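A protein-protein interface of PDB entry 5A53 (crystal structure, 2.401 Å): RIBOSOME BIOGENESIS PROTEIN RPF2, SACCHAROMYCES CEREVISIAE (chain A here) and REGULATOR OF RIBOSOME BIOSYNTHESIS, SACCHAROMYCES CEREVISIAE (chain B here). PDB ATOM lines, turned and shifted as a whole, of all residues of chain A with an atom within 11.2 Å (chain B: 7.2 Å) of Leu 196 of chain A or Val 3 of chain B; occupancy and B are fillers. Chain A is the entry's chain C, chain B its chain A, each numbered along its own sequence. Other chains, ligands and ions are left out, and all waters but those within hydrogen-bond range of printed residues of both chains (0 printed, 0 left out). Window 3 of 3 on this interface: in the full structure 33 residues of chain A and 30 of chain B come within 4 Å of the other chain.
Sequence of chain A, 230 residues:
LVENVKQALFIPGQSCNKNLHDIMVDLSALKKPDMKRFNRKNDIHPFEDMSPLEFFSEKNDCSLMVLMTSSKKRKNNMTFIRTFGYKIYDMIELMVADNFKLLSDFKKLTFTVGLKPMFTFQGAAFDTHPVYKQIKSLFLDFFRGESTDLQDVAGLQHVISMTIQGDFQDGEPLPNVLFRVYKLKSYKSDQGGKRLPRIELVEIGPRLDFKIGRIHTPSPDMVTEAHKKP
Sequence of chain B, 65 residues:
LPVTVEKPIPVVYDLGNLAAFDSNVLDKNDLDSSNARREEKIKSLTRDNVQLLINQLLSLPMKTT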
ATOM      1  N   VAL A 153      12.846 -19.277  21.100  1.00  0.00           N
ATOM      2  CA  VAL A 153      13.947 -19.813  21.896  1.00  0.00           C
ATOM      3  C   VAL A 153      13.449 -20.935  22.806  1.00  0.00           C
ATOM      4  O   VAL A 153      14.150 -21.920  23.042  1.00  0.00           O
ATOM      5  CB  VAL A 153      14.621 -18.704  22.736  1.00  0.00           C
ATOM      6  CG1 VAL A 153      15.576 -19.296  23.765  1.00  0.00           C
ATOM      7  CG2 VAL A 153      15.352 -17.727  21.828  1.00  0.00           C
ATOM      8  N   LEU A 156      13.657 -24.492  21.486  1.00  0.00           N
ATOM      9  CA  LEU A 156      14.943 -25.172  21.366  1.00  0.00           C
ATOM     10  C   LEU A 156      15.047 -26.256  22.432  1.00  0.00           C
ATOM     11  O   LEU A 156      15.606 -26.037  23.506  1.00  0.00           O
ATOM     12  CB  LEU A 156      16.095 -24.176  21.488  1.00  0.00           C
ATOM     13  CG  LEU A 156      16.120 -23.095  20.405  1.00  0.00           C
ATOM     14  CD1 LEU A 156      17.240 -22.098  20.655  1.00  0.00           C
ATOM     15  CD2 LEU A 156      16.252 -23.723  19.025  1.00  0.00           C
ATOM     16  N   LYS A 185      19.087 -28.655  28.794  1.00  0.00           N
ATOM     17  CA  LYS A 185      18.773 -27.973  30.043  1.00  0.00           C
ATOM     18  C   LYS A 185      19.672 -26.748  30.166  1.00  0.00           C
ATOM     19  O   LYS A 185      20.877 -26.829  29.925  1.00  0.00           O
ATOM     20  CB  LYS A 185      18.949 -28.900  31.247  1.00  0.00           C
ATOM     21  CG  LYS A 185      17.638 -29.336  31.894  1.00  0.00           C
ATOM     22  CD  LYS A 185      16.865 -28.144  32.449  1.00  0.00           C
ATOM     23  CE  LYS A 185      17.292 -27.815  33.873  1.00  0.00           C
ATOM     24  NZ  LYS A 185      16.547 -26.653  34.435  1.00  0.00           N
ATOM     25  N   SER A 186      19.085 -25.612  30.523  1.00  0.00           N
ATOM     26  CA  SER A 186      19.842 -24.368  30.598  1.00  0.00           C
ATOM     27  C   SER A 186      19.739 -23.716  31.973  1.00  0.00           C
ATOM     28  O   SER A 186      18.672 -23.691  32.584  1.00  0.00           O
ATOM     29  CB  SER A 186      19.369 -23.392  29.520  1.00  0.00           C
ATOM     30  OG  SER A 186      18.001 -23.070  29.689  1.00  0.00           O
ATOM     31  N   TYR A 187      20.863 -23.189  32.448  1.00  0.00           N
ATOM     32  CA  TYR A 187      20.916 -22.502  33.732  1.00  0.00           C
ATOM     33  C   TYR A 187      21.504 -21.107  33.555  1.00  0.00           C
ATOM     34  O   TYR A 187      22.131 -20.822  32.539  1.00  0.00           O
ATOM     35  CB  TYR A 187      21.741 -23.303  34.736  1.00  0.00           C
ATOM     36  CG  TYR A 187      21.360 -24.761  34.806  1.00  0.00           C
ATOM     37  CD1 TYR A 187      20.315 -25.187  35.614  1.00  0.00           C
ATOM     38  CD2 TYR A 187      22.046 -25.714  34.065  1.00  0.00           C
ATOM     39  CE1 TYR A 187      19.965 -26.518  35.684  1.00  0.00           C
ATOM     40  CE2 TYR A 187      21.704 -27.048  34.127  1.00  0.00           C
ATOM     41  CZ  TYR A 187      20.663 -27.445  34.937  1.00  0.00           C
ATOM     42  OH  TYR A 187      20.319 -28.775  35.000  1.00  0.00           O
ATOM     43  N   LYS A 188      21.311 -20.245  34.548  1.00  0.00           N
ATOM     44  CA  LYS A 188      21.743 -18.850  34.452  1.00  0.00           C
ATOM     45  C   LYS A 188      23.212 -18.716  34.859  1.00  0.00           C
ATOM     46  O   LYS A 188      23.688 -19.432  35.739  1.00  0.00           O
ATOM     47  CB  LYS A 188      20.861 -17.938  35.321  1.00  0.00           C
ATOM     48  CG  LYS A 188      19.473 -17.567  34.741  1.00  0.00           C
ATOM     49  CD  LYS A 188      18.922 -18.587  33.748  1.00  0.00           C
ATOM     50  CE  LYS A 188      17.818 -18.020  32.872  1.00  0.00           C
ATOM     51  NZ  LYS A 188      17.366 -19.033  31.875  1.00  0.00           N
ATOM     52  N   SER A 189      23.925 -17.800  34.210  1.00  0.00           N
ATOM     53  CA  SER A 189      25.352 -17.610  34.458  1.00  0.00           C
ATOM     54  C   SER A 189      25.596 -16.686  35.648  1.00  0.00           C
ATOM     55  O   SER A 189      26.656 -16.064  35.758  1.00  0.00           O
ATOM     56  CB  SER A 189      26.038 -17.052  33.209  1.00  0.00           C
ATOM     57  OG  SER A 189      25.768 -15.672  33.053  1.00  0.00           O
ATOM     58  N   ARG A 195      22.644 -11.687  27.777  1.00  0.00           N
ATOM     59  CA  ARG A 195      22.935 -12.751  28.731  1.00  0.00           C
ATOM     60  C   ARG A 195      22.896 -14.123  28.066  1.00  0.00           C
ATOM     61  O   ARG A 195      22.046 -14.389  27.217  1.00  0.00           O
ATOM     62  CB  ARG A 195      21.949 -12.703  29.900  1.00  0.00           C
ATOM     63  CG  ARG A 195      22.055 -11.445  30.748  1.00  0.00           C
ATOM     64  CD  ARG A 195      23.312 -11.464  31.605  1.00  0.00           C
ATOM     65  NE  ARG A 195      23.264 -12.509  32.623  1.00  0.00           N
ATOM     66  CZ  ARG A 195      24.286 -12.835  33.409  1.00  0.00           C
ATOM     67  NH1 ARG A 195      25.443 -12.199  33.296  1.00  0.00           N
ATOM     68  NH2 ARG A 195      24.151 -13.801  34.309  1.00  0.00           N
ATOM     69  N   LEU A 196      23.827 -14.987  28.458  1.00  0.00           N
ATOM     70  CA  LEU A 196      23.897 -16.342  27.923  1.00  0.00           C
ATOM     71  C   LEU A 196      23.711 -17.376  29.027  1.00  0.00           C
ATOM     72  O   LEU A 196      24.246 -17.221  30.125  1.00  0.00           O
ATOM     73  CB  LEU A 196      25.235 -16.575  27.218  1.00  0.00           C
ATOM     74  CG  LEU A 196      25.610 -15.642  26.065  1.00  0.00           C
ATOM     75  CD1 LEU A 196      27.063 -15.851  25.670  1.00  0.00           C
ATOM     76  CD2 LEU A 196      24.692 -15.862  24.874  1.00  0.00           C
ATOM     77  N   PRO A 197      22.945 -18.437  28.739  1.00  0.00           N
ATOM     78  CA  PRO A 197      22.751 -19.522  29.705  1.00  0.00           C
ATOM     79  C   PRO A 197      23.827 -20.601  29.606  1.00  0.00           C
ATOM     80  O   PRO A 197      24.400 -20.809  28.536  1.00  0.00           O
ATOM     81  CB  PRO A 197      21.386 -20.084  29.312  1.00  0.00           C
ATOM     82  CG  PRO A 197      21.337 -19.885  27.833  1.00  0.00           C
ATOM     83  CD  PRO A 197      22.088 -18.602  27.551  1.00  0.00           C
ATOM     84  N   ARG A 198      24.101 -21.273  30.719  1.00  0.00           N
ATOM     85  CA  ARG A 198      24.971 -22.442  30.709  1.00  0.00           C
ATOM     86  C   ARG A 198      24.165 -23.662  30.280  1.00  0.00           C
ATOM     87  O   ARG A 198      23.109 -23.945  30.846  1.00  0.00           O
ATOM     88  CB  ARG A 198      25.602 -22.668  32.083  1.00  0.00           C
ATOM     89  CG  ARG A 198      26.186 -24.062  32.283  1.00  0.00           C
ATOM     90  CD  ARG A 198      27.552 -24.214  31.630  1.00  0.00           C
ATOM     91  NE  ARG A 198      28.063 -25.576  31.767  1.00  0.00           N
ATOM     92  CZ  ARG A 198      29.284 -25.962  31.407  1.00  0.00           C
ATOM     93  NH1 ARG A 198      30.134 -25.086  30.889  1.00  0.00           N
ATOM     94  NH2 ARG A 198      29.655 -27.224  31.570  1.00  0.00           N
ATOM     95  N   ILE A 199      24.663 -24.380  29.281  1.00  0.00           N
ATOM     96  CA  ILE A 199      23.927 -25.503  28.713  1.00  0.00           C
ATOM     97  C   ILE A 199      24.422 -26.848  29.236  1.00  0.00           C
ATOM     98  O   ILE A 199      25.626 -27.091  29.313  1.00  0.00           O
ATOM     99  CB  ILE A 199      24.015 -25.500  27.171  1.00  0.00           C
ATOM    100  CG1 ILE A 199      23.446 -24.196  26.609  1.00  0.00           C
ATOM    101  CG2 ILE A 199      23.279 -26.694  26.582  1.00  0.00           C
ATOM    102  CD1 ILE A 199      21.974 -23.999  26.897  1.00  0.00           C
ATOM    103  N   GLU A 200      23.482 -27.710  29.609  1.00  0.00           N
ATOM    104  CA  GLU A 200      23.783 -29.094  29.951  1.00  0.00           C
ATOM    105  C   GLU A 200      22.882 -30.017  29.135  1.00  0.00           C
ATOM    106  O   GLU A 200      21.832 -29.596  28.652  1.00  0.00           O
ATOM    107  CB  GLU A 200      23.597 -29.342  31.450  1.00  0.00           C
ATOM    108  CG  GLU A 200      24.503 -28.501  32.338  1.00  0.00           C
ATOM    109  CD  GLU A 200      25.971 -28.865  32.193  1.00  0.00           C
ATOM    110  OE1 GLU A 200      26.268 -30.025  31.838  1.00  0.00           O
ATOM    111  OE2 GLU A 200      26.827 -27.989  32.433  1.00  0.00           O
ATOM    112  N   LEU B   1      29.632 -23.521  34.888  1.00  0.00           N
ATOM    113  CA  LEU B   1      29.217 -22.130  34.710  1.00  0.00           C
ATOM    114  C   LEU B   1      29.888 -21.356  33.553  1.00  0.00           C
ATOM    115  O   LEU B   1      29.309 -20.381  33.076  1.00  0.00           O
ATOM    116  CB  LEU B   1      29.420 -21.349  36.015  1.00  0.00           C
ATOM    117  CG  LEU B   1      28.268 -21.389  37.031  1.00  0.00           C
ATOM    118  CD1 LEU B   1      28.089 -22.774  37.653  1.00  0.00           C
ATOM    119  CD2 LEU B   1      28.436 -20.320  38.109  1.00  0.00           C
ATOM    120  N   PRO B   2      31.102 -21.754  33.109  1.00  0.00           N
ATOM    121  CA  PRO B   2      31.590 -21.063  31.906  1.00  0.00           C
ATOM    122  C   PRO B   2      30.692 -21.261  30.683  1.00  0.00           C
ATOM    123  O   PRO B   2      30.236 -22.376  30.420  1.00  0.00           O
ATOM    124  CB  PRO B   2      32.963 -21.698  31.668  1.00  0.00           C
ATOM    125  CG  PRO B   2      33.410 -22.122  33.013  1.00  0.00           C
ATOM    126  CD  PRO B   2      32.168 -22.562  33.733  1.00  0.00           C
ATOM    127  N   VAL B   3      30.447 -20.181  29.947  1.00  0.00           N
ATOM    128  CA  VAL B   3      29.578 -20.226  28.778  1.00  0.00           C
ATOM    129  C   VAL B   3      30.371 -20.142  27.476  1.00  0.00           C
ATOM    130  O   VAL B   3      29.808 -20.258  26.388  1.00  0.00           O
ATOM    131  CB  VAL B   3      28.540 -19.088  28.802  1.00  0.00           C
ATOM    132  CG1 VAL B   3      27.598 -19.256  29.984  1.00  0.00           C
ATOM    133  CG2 VAL B   3      29.235 -17.736  28.851  1.00  0.00           C
ATOM    134  N   THR B   4      31.679 -19.939  27.592  1.00  0.00           N
ATOM    135  CA  THR B   4      32.548 -19.901  26.420  1.00  0.00           C
ATOM    136  C   THR B   4      33.260 -21.236  26.222  1.00  0.00           C
ATOM    137  O   THR B   4      33.494 -21.975  27.177  1.00  0.00           O
ATOM    138  CB  THR B   4      33.600 -18.779  26.523  1.00  0.00           C
ATOM    139  OG1 THR B   4      34.158 -18.761  27.843  1.00  0.00           O
ATOM    140  CG2 THR B   4      32.967 -17.428  26.233  1.00  0.00           C
ATOM    141  N   VAL B   5      33.590 -21.540  24.972  1.00  0.00           N
ATOM    142  CA  VAL B   5      34.292 -22.774  24.634  1.00  0.00           C
ATOM    143  C   VAL B   5      35.463 -22.483  23.703  1.00  0.00           C
ATOM    144  O   VAL B   5      35.288 -21.868  22.652  1.00  0.00           O
ATOM    145  CB  VAL B   5      33.356 -23.799  23.959  1.00  0.00           C
ATOM    146  CG1 VAL B   5      34.127 -25.056  23.584  1.00  0.00           C
ATOM    147  CG2 VAL B   5      32.181 -24.140  24.867  1.00  0.00           C
ATOM    148  N   ARG B  47      27.930 -31.212  24.139  1.00  0.00           N
ATOM    149  CA  ARG B  47      27.524 -30.096  24.989  1.00  0.00           C
ATOM    150  C   ARG B  47      28.268 -28.816  24.624  1.00  0.00           C
ATOM    151  O   ARG B  47      27.691 -27.729  24.631  1.00  0.00           O
ATOM    152  CB  ARG B  47      27.760 -30.435  26.462  1.00  0.00           C
ATOM    153  CG  ARG B  47      27.060 -29.501  27.434  1.00  0.00           C
ATOM    154  CD  ARG B  47      27.991 -29.068  28.554  1.00  0.00           C
ATOM    155  NE  ARG B  47      29.068 -28.211  28.065  1.00  0.00           N
ATOM    156  CZ  ARG B  47      28.985 -26.888  27.970  1.00  0.00           C
ATOM    157  NH1 ARG B  47      27.872 -26.264  28.333  1.00  0.00           N
ATOM    158  NH2 ARG B  47      30.014 -26.187  27.515  1.00  0.00           N
ATOM    159  N   ASP B  48      29.552 -28.954  24.304  1.00  0.00           N
ATOM    160  CA  ASP B  48      30.370 -27.814  23.913  1.00  0.00           C
ATOM    161  C   ASP B  48      29.865 -27.186  22.619  1.00  0.00           C
ATOM    162  O   ASP B  48      29.794 -25.962  22.497  1.00  0.00           O
ATOM    163  CB  ASP B  48      31.834 -28.233  23.755  1.00  0.00           C
ATOM    164  CG  ASP B  48      32.512 -28.501  25.084  1.00  0.00           C
ATOM    165  OD1 ASP B  48      31.939 -28.132  26.132  1.00  0.00           O
ATOM    166  OD2 ASP B  48      33.621 -29.075  25.081  1.00  0.00           O
ATOM    167  N   GLN B  51      26.474 -25.533  23.161  1.00  0.00           N
ATOM    168  CA  GLN B  51      26.729 -24.263  23.833  1.00  0.00           C
ATOM    169  C   GLN B  51      27.118 -23.188  22.823  1.00  0.00           C
ATOM    170  O   GLN B  51      26.563 -22.090  22.828  1.00  0.00           O
ATOM    171  CB  GLN B  51      27.829 -24.424  24.885  1.00  0.00           C
ATOM    172  CG  GLN B  51      28.132 -23.156  25.668  1.00  0.00           C
ATOM    173  CD  GLN B  51      27.060 -22.827  26.687  1.00  0.00           C
ATOM    174  OE1 GLN B  51      26.853 -23.569  27.648  1.00  0.00           O
ATOM    175  NE2 GLN B  51      26.371 -21.710  26.483  1.00  0.00           N
ATOM    176  N   LEU B  52      28.071 -23.518  21.956  1.00  0.00           N
ATOM    177  CA  LEU B  52      28.516 -22.601  20.912  1.00  0.00           C
ATOM    178  C   LEU B  52      27.385 -22.281  19.939  1.00  0.00           C
ATOM    179  O   LEU B  52      27.264 -21.151  19.464  1.00  0.00           O
ATOM    180  CB  LEU B  52      29.708 -23.188  20.154  1.00  0.00           C
ATOM    181  CG  LEU B  52      31.035 -23.281  20.910  1.00  0.00           C
ATOM    182  CD1 LEU B  52      32.016 -24.159  20.152  1.00  0.00           C
ATOM    183  CD2 LEU B  52      31.624 -21.896  21.138  1.00  0.00           C
ATOM    184  N   ILE B  54      24.060 -22.372  20.620  1.00  0.00           N
ATOM    185  CA  ILE B  54      23.098 -21.532  21.330  1.00  0.00           C
ATOM    186  C   ILE B  54      23.598 -20.093  21.446  1.00  0.00           C
ATOM    187  O   ILE B  54      22.831 -19.146  21.265  1.00  0.00           O
ATOM    188  CB  ILE B  54      22.796 -22.094  22.735  1.00  0.00           C
ATOM    189  CG1 ILE B  54      21.961 -23.372  22.625  1.00  0.00           C
ATOM    190  CG2 ILE B  54      22.062 -21.070  23.584  1.00  0.00           C
ATOM    191  CD1 ILE B  54      20.549 -23.139  22.126  1.00  0.00           C
ATOM    192  N   ASN B  55      24.887 -19.934  21.738  1.00  0.00           N
ATOM    193  CA  ASN B  55      25.509 -18.614  21.782  1.00  0.00           C
ATOM    194  C   ASN B  55      25.311 -17.848  20.475  1.00  0.00           C
ATOM    195  O   ASN B  55      24.926 -16.680  20.481  1.00  0.00           O
ATOM    196  CB  ASN B  55      27.004 -18.733  22.088  1.00  0.00           C
ATOM    197  CG  ASN B  55      27.278 -19.159  23.518  1.00  0.00           C
ATOM    198  OD1 ASN B  55      26.356 -19.381  24.303  1.00  0.00           O
ATOM    199  ND2 ASN B  55      28.555 -19.277  23.863  1.00  0.00           N
ATOM    200  N   GLN B  56      25.571 -18.521  19.358  1.00  0.00           N
ATOM    201  CA  GLN B  56      25.405 -17.924  18.037  1.00  0.00           C
ATOM    202  C   GLN B  56      23.948 -17.574  17.752  1.00  0.00           C
ATOM    203  O   GLN B  56      23.653 -16.528  17.173  1.00  0.00           O
ATOM    204  CB  GLN B  56      25.931 -18.870  16.957  1.00  0.00           C
ATOM    205  CG  GLN B  56      27.439 -19.043  16.963  1.00  0.00           C
ATOM    206  CD  GLN B  56      28.160 -17.888  16.298  1.00  0.00           C
ATOM    207  OE1 GLN B  56      27.554 -17.097  15.575  1.00  0.00           O
ATOM    208  NE2 GLN B  56      29.463 -17.788  16.534  1.00  0.00           N
ATOM    209  N   LEU B  58      21.595 -16.850  19.924  1.00  0.00           N
ATOM    210  CA  LEU B  58      21.139 -15.758  20.779  1.00  0.00           C
ATOM    211  C   LEU B  58      21.765 -14.420  20.393  1.00  0.00           C
ATOM    212  O   LEU B  58      21.447 -13.389  20.985  1.00  0.00           O
ATOM    213  CB  LEU B  58      21.438 -16.072  22.245  1.00  0.00           C
ATOM    214  CG  LEU B  58      20.661 -17.249  22.839  1.00  0.00           C
ATOM    215  CD1 LEU B  58      20.972 -17.406  24.318  1.00  0.00           C
ATOM    216  CD2 LEU B  58      19.164 -17.075  22.618  1.00  0.00           C
ATOM    217  N   SER B  59      22.650 -14.438  19.402  1.00  0.00           N
ATOM    218  CA  SER B  59      23.267 -13.211  18.909  1.00  0.00           C
ATOM    219  C   SER B  59      22.582 -12.741  17.628  1.00  0.00           C
ATOM    220  O   SER B  59      22.910 -11.687  17.084  1.00  0.00           O
ATOM    221  CB  SER B  59      24.763 -13.417  18.669  1.00  0.00           C
ATOM    222  OG  SER B  59      24.988 -14.314  17.595  1.00  0.00           O
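Among the printed residues, pairs that only touch across the chains: Val 153 of chain A with Leu 58 of chain B (3.9 Å), Leu 156 of chain A with Ile 54 of chain B (3.8 Å), Leu 196 of chain A with Val 3 of chain B (3.9 Å), Leu 196 of chain A with Asn 55 of chain B (3.9 Å), Pro 197 of chain A with Val 3 of chain B (3.8 Å), Pro 197 of chain A with Leu 58 of chain B (3.6 Å), Arg 198 of chain A with Leu 1 of chain B (3.9 Å), Arg 198 of chain A with Arg 47 of chain B (3.4 Å), Arg 198 of chain A with Gln 51 of chain B (3.8 Å) and Glu 200 of chain A with Arg 47 of chain B (3.8 Å).
The guanidinium group (NH1) of Arg 198 of chain A is in hydrogen-bond range of the backbone carbonyl oxygen (O) of Pro 2 of chain B, 2.8 Å away. NH1 of Arg 47 of chain B lies within hydrogen-bond range of O of Ile 199 of chain A, at 2.6 Å. NE2 of Gln 51 of chain B is in hydrogen-bond range of O of Pro 197 of chain A, at 3.0 Å. The side-chain amide oxygen (OE1) of Gln 51 of chain B sits at hydrogen-bond distance from the backbone NH (N) of Ile 199 of chain A, 2.8 Å away.
Leu 196 of chain A touches two residues of chain B. Of chain A, only Leu 196 (3.9 Å) and Pro 197 (3.8 Å) come within 4 Å of Val 3 of chain B. Of chain A, only Arg 198 comes within 4 Å of Pro 2 of chain B. No residue of chain A comes within 4 Å of Thr 4 of chain B. No residue of chain A comes within 4 Å of Val 5 of chain B. Leu 58 of chain B touches just these residues of chain A: Val 153 and Pro 197. Printed residues of chain B within 4 Å of Val 153 of chain A: Leu 58 (3.9 Å). Of the printed residues of chain A, Ile 54 of chain B touches Leu 156. Arg 195 of chain A touches none of the printed residues of chain B. Asp 48 of chain B touches none of the printed residues of chain A. The nearest residue of chain A that does not touch Val 3 of chain B is Arg 198 of chain A (4.1 Å).
The backbone carbonyl oxygen (O) of Val 3 of chain B is in hydrogen-bond range of the side-chain amide nitrogen (ND2) of Asn 55 of chain B (3.0 Å). The guanidinium group (NH2) of Arg 47 of chain B is in salt-bridge range of the side-chain carboxylate (OD1) of Asp 48 of chain B (3.1 Å). The guanidinium group of Arg 47 of chain B is in hydrogen-bond range of the side-chain amide oxygen of Gln 51 of chain B (3.0 Å). N of Glu 200 of chain A is in hydrogen-bond range of O of Lys 185 of chain A (2.8 Å). The backbone NH (N) of Arg 198 of chain A lies within hydrogen-bond range of the backbone carbonyl oxygen (O) of Tyr 187 of chain A. NE of Arg 198 of chain A is in salt-bridge range of OE2 of Glu 200 of chain A.
Hydrophobic or aromatic side chains of chain A that line the printed part of chain B: Val 153, Leu 156, Leu 196, Pro 197 and Ile 199. Of the 14 printed residues of chain B, 8 touch a printed residue of chain A. Hydrophobic or aromatic side chains of chain B that line the printed part of chain A: Val 3, Ile 54 and Leu 58. Among the printed residues, no Asp or Glu carboxylate lies within 4 Å of a Lys or Arg side-chain nitrogen of the other chain.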
